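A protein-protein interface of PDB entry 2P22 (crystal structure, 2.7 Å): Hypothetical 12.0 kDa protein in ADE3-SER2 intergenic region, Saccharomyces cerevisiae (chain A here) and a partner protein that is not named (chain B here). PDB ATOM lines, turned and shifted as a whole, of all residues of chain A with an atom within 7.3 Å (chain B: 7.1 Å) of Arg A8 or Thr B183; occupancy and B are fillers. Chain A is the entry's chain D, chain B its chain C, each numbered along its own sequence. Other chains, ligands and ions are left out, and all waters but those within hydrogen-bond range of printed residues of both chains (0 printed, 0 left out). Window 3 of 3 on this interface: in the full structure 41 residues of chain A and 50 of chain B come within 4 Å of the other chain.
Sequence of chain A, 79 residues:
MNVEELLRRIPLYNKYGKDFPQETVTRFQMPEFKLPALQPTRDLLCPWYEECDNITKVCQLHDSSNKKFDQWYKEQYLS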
ATOM      1  N   MET A   1      33.943  34.804  22.745  1.00  0.00           N
ATOM      2  CA  MET A   1      34.675  33.669  22.111  1.00  0.00           C
ATOM      3  C   MET A   1      35.213  32.739  23.192  1.00  0.00           C
ATOM      4  O   MET A   1      35.068  31.524  23.108  1.00  0.00           O
ATOM      5  CB  MET A   1      35.842  34.193  21.269  1.00  0.00           C
ATOM      6  CG  MET A   1      36.217  33.298  20.093  1.00  0.00           C
ATOM      7  SD  MET A   1      36.452  31.558  20.529  1.00  0.00           S
ATOM      8  CE  MET A   1      34.887  30.836  19.969  1.00  0.00           C
ATOM      9  N   ASN A   2      35.842  33.321  24.203  1.00  0.00           N
ATOM     10  CA  ASN A   2      36.398  32.549  25.300  1.00  0.00           C
ATOM     11  C   ASN A   2      35.313  31.695  25.942  1.00  0.00           C
ATOM     12  O   ASN A   2      35.434  30.471  26.011  1.00  0.00           O
ATOM     13  CB  ASN A   2      37.004  33.493  26.339  1.00  0.00           C
ATOM     14  CG  ASN A   2      37.744  32.757  27.433  1.00  0.00           C
ATOM     15  OD1 ASN A   2      37.133  32.121  28.288  1.00  0.00           O
ATOM     16  ND2 ASN A   2      39.070  32.835  27.408  1.00  0.00           N
ATOM     17  N   VAL A   3      34.247  32.342  26.400  1.00  0.00           N
ATOM     18  CA  VAL A   3      33.146  31.630  27.038  1.00  0.00           C
ATOM     19  C   VAL A   3      32.364  30.843  26.003  1.00  0.00           C
ATOM     20  O   VAL A   3      31.943  29.710  26.250  1.00  0.00           O
ATOM     21  CB  VAL A   3      32.183  32.597  27.729  1.00  0.00           C
ATOM     22  CG1 VAL A   3      31.211  31.813  28.597  1.00  0.00           C
ATOM     23  CG2 VAL A   3      32.965  33.598  28.558  1.00  0.00           C
ATOM     24  N   GLU A   4      32.163  31.470  24.848  1.00  0.00           N
ATOM     25  CA  GLU A   4      31.450  30.860  23.732  1.00  0.00           C
ATOM     26  C   GLU A   4      32.069  29.495  23.428  1.00  0.00           C
ATOM     27  O   GLU A   4      31.382  28.473  23.361  1.00  0.00           O
ATOM     28  CB  GLU A   4      31.582  31.748  22.496  1.00  0.00           C
ATOM     29  CG  GLU A   4      30.274  32.202  21.893  1.00  0.00           C
ATOM     30  CD  GLU A   4      29.513  33.138  22.802  1.00  0.00           C
ATOM     31  OE1 GLU A   4      30.117  34.123  23.281  1.00  0.00           O
ATOM     32  OE2 GLU A   4      28.307  32.894  23.023  1.00  0.00           O
ATOM     33  N   GLU A   5      33.384  29.505  23.243  1.00  0.00           N
ATOM     34  CA  GLU A   5      34.142  28.308  22.937  1.00  0.00           C
ATOM     35  C   GLU A   5      33.984  27.271  24.033  1.00  0.00           C
ATOM     36  O   GLU A   5      33.586  26.137  23.764  1.00  0.00           O
ATOM     37  CB  GLU A   5      35.617  28.665  22.767  1.00  0.00           C
ATOM     38  CG  GLU A   5      36.420  27.585  22.077  1.00  0.00           C
ATOM     39  CD  GLU A   5      37.869  27.975  21.853  1.00  0.00           C
ATOM     40  OE1 GLU A   5      38.608  27.166  21.244  1.00  0.00           O
ATOM     41  OE2 GLU A   5      38.261  29.085  22.288  1.00  0.00           O
ATOM     42  N   LEU A   6      34.293  27.665  25.267  1.00  0.00           N
ATOM     43  CA  LEU A   6      34.181  26.772  26.420  1.00  0.00           C
ATOM     44  C   LEU A   6      32.829  26.066  26.428  1.00  0.00           C
ATOM     45  O   LEU A   6      32.770  24.844  26.548  1.00  0.00           O
ATOM     46  CB  LEU A   6      34.363  27.557  27.730  1.00  0.00           C
ATOM     47  CG  LEU A   6      34.562  26.756  29.035  1.00  0.00           C
ATOM     48  CD1 LEU A   6      35.157  27.661  30.106  1.00  0.00           C
ATOM     49  CD2 LEU A   6      33.251  26.156  29.518  1.00  0.00           C
ATOM     50  N   LEU A   7      31.750  26.834  26.294  1.00  0.00           N
ATOM     51  CA  LEU A   7      30.407  26.269  26.295  1.00  0.00           C
ATOM     52  C   LEU A   7      30.217  25.175  25.250  1.00  0.00           C
ATOM     53  O   LEU A   7      29.817  24.053  25.587  1.00  0.00           O
ATOM     54  CB  LEU A   7      29.364  27.370  26.078  1.00  0.00           C
ATOM     55  CG  LEU A   7      29.121  28.326  27.255  1.00  0.00           C
ATOM     56  CD1 LEU A   7      28.304  29.532  26.817  1.00  0.00           C
ATOM     57  CD2 LEU A   7      28.409  27.563  28.365  1.00  0.00           C
ATOM     58  N   ARG A   8      30.509  25.506  23.989  1.00  0.00           N
ATOM     59  CA  ARG A   8      30.357  24.572  22.871  1.00  0.00           C
ATOM     60  C   ARG A   8      31.399  23.473  22.909  1.00  0.00           C
ATOM     61  O   ARG A   8      31.209  22.405  22.334  1.00  0.00           O
ATOM     62  CB  ARG A   8      30.444  25.307  21.520  1.00  0.00           C
ATOM     63  CG  ARG A   8      31.814  25.914  21.196  1.00  0.00           C
ATOM     64  CD  ARG A   8      31.855  26.503  19.776  1.00  0.00           C
ATOM     65  NE  ARG A   8      30.816  27.510  19.548  1.00  0.00           N
ATOM     66  CZ  ARG A   8      31.030  28.822  19.463  1.00  0.00           C
ATOM     67  NH1 ARG A   8      32.260  29.317  19.585  1.00  0.00           N
ATOM     68  NH2 ARG A   8      30.001  29.637  19.258  1.00  0.00           N
ATOM     69  N   ARG A   9      32.505  23.733  23.583  1.00  0.00           N
ATOM     70  CA  ARG A   9      33.553  22.736  23.673  1.00  0.00           C
ATOM     71  C   ARG A   9      33.166  21.638  24.642  1.00  0.00           C
ATOM     72  O   ARG A   9      33.816  20.599  24.701  1.00  0.00           O
ATOM     73  CB  ARG A   9      34.874  23.394  24.081  1.00  0.00           C
ATOM     74  CG  ARG A   9      35.816  23.673  22.890  1.00  0.00           C
ATOM     75  CD  ARG A   9      35.080  24.289  21.677  1.00  0.00           C
ATOM     76  NE  ARG A   9      35.982  24.647  20.574  1.00  0.00           N
ATOM     77  CZ  ARG A   9      35.589  25.065  19.368  1.00  0.00           C
ATOM     78  NH1 ARG A   9      34.301  25.181  19.079  1.00  0.00           N
ATOM     79  NH2 ARG A   9      36.488  25.384  18.448  1.00  0.00           N
ATOM     80  N   ILE A  10      32.098  21.870  25.398  1.00  0.00           N
ATOM     81  CA  ILE A  10      31.619  20.875  26.354  1.00  0.00           C
ATOM     82  C   ILE A  10      30.270  20.366  25.890  1.00  0.00           C
ATOM     83  O   ILE A  10      29.354  21.149  25.652  1.00  0.00           O
ATOM     84  CB  ILE A  10      31.452  21.455  27.754  1.00  0.00           C
ATOM     85  CG1 ILE A  10      32.793  21.985  28.262  1.00  0.00           C
ATOM     86  CG2 ILE A  10      30.896  20.386  28.687  1.00  0.00           C
ATOM     87  CD1 ILE A  10      32.688  22.744  29.575  1.00  0.00           C
ATOM     88  N   PRO A  11      30.126  19.036  25.785  1.00  0.00           N
ATOM     89  CA  PRO A  11      28.907  18.347  25.343  1.00  0.00           C
ATOM     90  C   PRO A  11      27.662  18.470  26.224  1.00  0.00           C
ATOM     91  O   PRO A  11      27.735  18.438  27.454  1.00  0.00           O
ATOM     92  CB  PRO A  11      29.373  16.901  25.205  1.00  0.00           C
ATOM     93  CG  PRO A  11      30.370  16.774  26.323  1.00  0.00           C
ATOM     94  CD  PRO A  11      31.157  18.061  26.201  1.00  0.00           C
ATOM     95  N   LEU A  12      26.514  18.614  25.570  1.00  0.00           N
ATOM     96  CA  LEU A  12      25.235  18.715  26.260  1.00  0.00           C
ATOM     97  C   LEU A  12      24.778  17.325  26.656  1.00  0.00           C
ATOM     98  O   LEU A  12      25.184  16.329  26.051  1.00  0.00           O
ATOM     99  CB  LEU A  12      24.175  19.333  25.347  1.00  0.00           C
ATOM    100  CG  LEU A  12      24.357  20.802  24.974  1.00  0.00           C
ATOM    101  CD1 LEU A  12      23.165  21.287  24.151  1.00  0.00           C
ATOM    102  CD2 LEU A  12      24.480  21.617  26.245  1.00  0.00           C
ATOM    103  N   ARG B 177      18.667  28.963  23.307  1.00  0.00           N
ATOM    104  CA  ARG B 177      18.541  27.788  22.442  1.00  0.00           C
ATOM    105  C   ARG B 177      19.516  27.794  21.275  1.00  0.00           C
ATOM    106  O   ARG B 177      20.047  26.747  20.930  1.00  0.00           O
ATOM    107  CB  ARG B 177      17.108  27.656  21.942  1.00  0.00           C
ATOM    108  CG  ARG B 177      16.161  27.340  23.061  1.00  0.00           C
ATOM    109  CD  ARG B 177      14.724  27.434  22.637  1.00  0.00           C
ATOM    110  NE  ARG B 177      13.882  26.936  23.707  1.00  0.00           N
ATOM    111  CZ  ARG B 177      13.816  27.481  24.915  1.00  0.00           C
ATOM    112  NH1 ARG B 177      14.539  28.557  25.204  1.00  0.00           N
ATOM    113  NH2 ARG B 177      13.049  26.924  25.845  1.00  0.00           N
ATOM    114  N   ARG B 178      19.756  28.963  20.677  1.00  0.00           N
ATOM    115  CA  ARG B 178      20.711  29.053  19.575  1.00  0.00           C
ATOM    116  C   ARG B 178      22.085  28.560  20.023  1.00  0.00           C
ATOM    117  O   ARG B 178      22.719  27.783  19.320  1.00  0.00           O
ATOM    118  CB  ARG B 178      20.827  30.492  19.043  1.00  0.00           C
ATOM    119  CG  ARG B 178      21.799  30.652  17.858  1.00  0.00           C
ATOM    120  CD  ARG B 178      21.182  31.428  16.680  1.00  0.00           C
ATOM    121  NE  ARG B 178      21.236  32.898  16.779  1.00  0.00           N
ATOM    122  CZ  ARG B 178      22.319  33.648  16.560  1.00  0.00           C
ATOM    123  NH1 ARG B 178      23.474  33.078  16.239  1.00  0.00           N
ATOM    124  NH2 ARG B 178      22.235  34.978  16.602  1.00  0.00           N
ATOM    125  N   GLU B 179      22.548  28.993  21.193  1.00  0.00           N
ATOM    126  CA  GLU B 179      23.858  28.551  21.661  1.00  0.00           C
ATOM    127  C   GLU B 179      23.800  27.081  22.043  1.00  0.00           C
ATOM    128  O   GLU B 179      24.781  26.355  21.908  1.00  0.00           O
ATOM    129  CB  GLU B 179      24.357  29.434  22.826  1.00  0.00           C
ATOM    130  CG  GLU B 179      23.439  29.527  24.027  1.00  0.00           C
ATOM    131  CD  GLU B 179      23.808  30.666  24.976  1.00  0.00           C
ATOM    132  OE1 GLU B 179      23.614  31.847  24.615  1.00  0.00           O
ATOM    133  OE2 GLU B 179      24.292  30.382  26.088  1.00  0.00           O
ATOM    134  N   LYS B 180      22.639  26.634  22.500  1.00  0.00           N
ATOM    135  CA  LYS B 180      22.464  25.228  22.859  1.00  0.00           C
ATOM    136  C   LYS B 180      22.686  24.358  21.619  1.00  0.00           C
ATOM    137  O   LYS B 180      23.346  23.312  21.670  1.00  0.00           O
ATOM    138  CB  LYS B 180      21.047  24.996  23.370  1.00  0.00           C
ATOM    139  CG  LYS B 180      20.815  25.420  24.780  1.00  0.00           C
ATOM    140  CD  LYS B 180      21.474  24.437  25.714  1.00  0.00           C
ATOM    141  CE  LYS B 180      20.705  24.335  27.028  1.00  0.00           C
ATOM    142  NZ  LYS B 180      19.295  23.867  26.818  1.00  0.00           N
ATOM    143  N   LEU B 181      22.118  24.806  20.504  1.00  0.00           N
ATOM    144  CA  LEU B 181      22.222  24.081  19.241  1.00  0.00           C
ATOM    145  C   LEU B 181      23.660  24.075  18.751  1.00  0.00           C
ATOM    146  O   LEU B 181      24.152  23.066  18.250  1.00  0.00           O
ATOM    147  CB  LEU B 181      21.300  24.721  18.195  1.00  0.00           C
ATOM    148  CG  LEU B 181      19.798  24.542  18.466  1.00  0.00           C
ATOM    149  CD1 LEU B 181      18.976  25.560  17.704  1.00  0.00           C
ATOM    150  CD2 LEU B 181      19.405  23.124  18.094  1.00  0.00           C
ATOM    151  N   ALA B 182      24.333  25.209  18.909  1.00  0.00           N
ATOM    152  CA  ALA B 182      25.717  25.335  18.492  1.00  0.00           C
ATOM    153  C   ALA B 182      26.529  24.236  19.151  1.00  0.00           C
ATOM    154  O   ALA B 182      27.362  23.596  18.513  1.00  0.00           O
ATOM    155  CB  ALA B 182      26.254  26.694  18.884  1.00  0.00           C
ATOM    156  N   THR B 183      26.270  24.010  20.434  1.00  0.00           N
ATOM    157  CA  THR B 183      26.988  22.982  21.174  1.00  0.00           C
ATOM    158  C   THR B 183      26.546  21.621  20.669  1.00  0.00           C
ATOM    159  O   THR B 183      27.373  20.746  20.408  1.00  0.00           O
ATOM    160  CB  THR B 183      26.702  23.076  22.694  1.00  0.00           C
ATOM    161  OG1 THR B 183      26.987  24.401  23.152  1.00  0.00           O
ATOM    162  CG2 THR B 183      27.573  22.102  23.463  1.00  0.00           C
ATOM    163  N   TRP B 184      25.237  21.448  20.522  1.00  0.00           N
ATOM    164  CA  TRP B 184      24.697  20.180  20.048  1.00  0.00           C
ATOM    165  C   TRP B 184      25.318  19.780  18.714  1.00  0.00           C
ATOM    166  O   TRP B 184      25.647  18.613  18.507  1.00  0.00           O
ATOM    167  CB  TRP B 184      23.177  20.271  19.896  1.00  0.00           C
ATOM    168  CG  TRP B 184      22.496  18.933  19.996  1.00  0.00           C
ATOM    169  CD1 TRP B 184      23.064  17.702  19.810  1.00  0.00           C
ATOM    170  CD2 TRP B 184      21.121  18.692  20.301  1.00  0.00           C
ATOM    171  NE1 TRP B 184      22.128  16.713  19.987  1.00  0.00           N
ATOM    172  CE2 TRP B 184      20.926  17.296  20.295  1.00  0.00           C
ATOM    173  CE3 TRP B 184      20.035  19.517  20.591  1.00  0.00           C
ATOM    174  CZ2 TRP B 184      19.693  16.713  20.553  1.00  0.00           C
ATOM    175  CZ3 TRP B 184      18.808  18.935  20.850  1.00  0.00           C
ATOM    176  CH2 TRP B 184      18.649  17.548  20.833  1.00  0.00           C
ATOM    177  N   ASP B 185      25.487  20.751  17.816  1.00  0.00           N
ATOM    178  CA  ASP B 185      26.060  20.492  16.491  1.00  0.00           C
ATOM    179  C   ASP B 185      27.487  19.942  16.509  1.00  0.00           C
ATOM    180  O   ASP B 185      28.180  19.967  15.496  1.00  0.00           O
ATOM    181  CB  ASP B 185      26.022  21.763  15.642  1.00  0.00           C
ATOM    182  CG  ASP B 185      24.609  22.171  15.267  1.00  0.00           C
ATOM    183  OD1 ASP B 185      24.435  23.275  14.700  1.00  0.00           O
ATOM    184  OD2 ASP B 185      23.671  21.384  15.535  1.00  0.00           O
ATOM    185  N   LYS B 186      27.926  19.456  17.663  1.00  0.00           N
ATOM    186  CA  LYS B 186      29.254  18.875  17.786  1.00  0.00           C
ATOM    187  C   LYS B 186      29.129  17.657  18.686  1.00  0.00           C
ATOM    188  O   LYS B 186      29.954  17.442  19.573  1.00  0.00           O
ATOM    189  CB  LYS B 186      30.233  19.875  18.402  1.00  0.00           C
ATOM    190  CG  LYS B 186      30.383  21.167  17.627  1.00  0.00           C
ATOM    191  CD  LYS B 186      31.370  22.115  18.305  1.00  0.00           C
ATOM    192  CE  LYS B 186      32.781  21.535  18.349  1.00  0.00           C
ATOM    193  NZ  LYS B 186      33.788  22.500  18.894  1.00  0.00           N
ATOM    194  N   GLN B 187      28.077  16.873  18.459  1.00  0.00           N
ATOM    195  CA  GLN B 187      27.814  15.666  19.249  1.00  0.00           C
ATOM    196  C   GLN B 187      26.476  14.981  18.886  1.00  0.00           C
ATOM    197  O   GLN B 187      25.802  15.354  17.923  1.00  0.00           O
ATOM    198  CB  GLN B 187      27.825  16.003  20.758  1.00  0.00           C
ATOM    199  CG  GLN B 187      27.236  17.374  21.113  1.00  0.00           C
ATOM    200  CD  GLN B 187      26.458  17.380  22.415  1.00  0.00           C
ATOM    201  OE1 GLN B 187      25.996  18.434  22.868  1.00  0.00           O
ATOM    202  NE2 GLN B 187      26.299  16.205  23.020  1.00  0.00           N
ATOM    203  N   GLY B 188      26.113  13.968  19.669  1.00  0.00           N
ATOM    204  CA  GLY B 188      24.866  13.264  19.460  1.00  0.00           C
ATOM    205  C   GLY B 188      23.964  13.610  20.627  1.00  0.00           C
ATOM    206  O   GLY B 188      22.813  13.997  20.423  1.00  0.00           O
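Of the printed residues of chain B, Leu A7 touches Thr B183 (3.7 Å). Arg A8 touches just one residue of chain B: Thr B183 (3.4 Å). Of the printed residues of chain B, Arg A9 touches Lys B186. Of the printed residues of chain A, Lys B180 touches Leu A12. Thr B183 touches just these residues of chain A: Leu A7 (3.7 Å), Arg A8 (3.4 Å), Ile A10 (3.0 Å) and Leu A12 (3.8 Å). Printed residues of chain A within 4 Å of Lys B186: Arg A9 (2.7 Å). Of the printed residues of chain A, Gln B187 touches Pro A11 (3.7 Å) and Leu A12 (2.8 Å).
Among the printed residues, 8 pairs touch across the chains. Among the printed residues, no Asp or Glu carboxylate lies within 4 Å of a Lys or Arg side-chain nitrogen of the other chain.
NH1 of Arg A9 sits close to NZ of Lys B186, at 2.7 Å. The side-chain amide oxygen (OE1) of Gln B187 sits at hydrogen-bond distance from the backbone NH (N) of Leu A12 (2.8 Å).
The backbone carbonyl oxygen (O) of Glu B179 sits at hydrogen-bond distance from the side-chain hydroxyl (OG1) of Thr B183, at 3.2 Å. The side-chain carboxylate (OE1) of Glu A5 lies within salt-bridge range of the guanidinium group (NE) of Arg A9, 3.7 Å away.
O of Leu A7 touches CG2 of Thr B183, 3.7 Å away. OG1 of Thr B183 touches CA of Arg A8 (3.4 Å). Thr B183 touches Ile A10 (CG2 to O, 3.0 Å). Pro A11 touches Gln B187. Leu A12 touches Lys B180. Thr B183 touches Leu A12.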
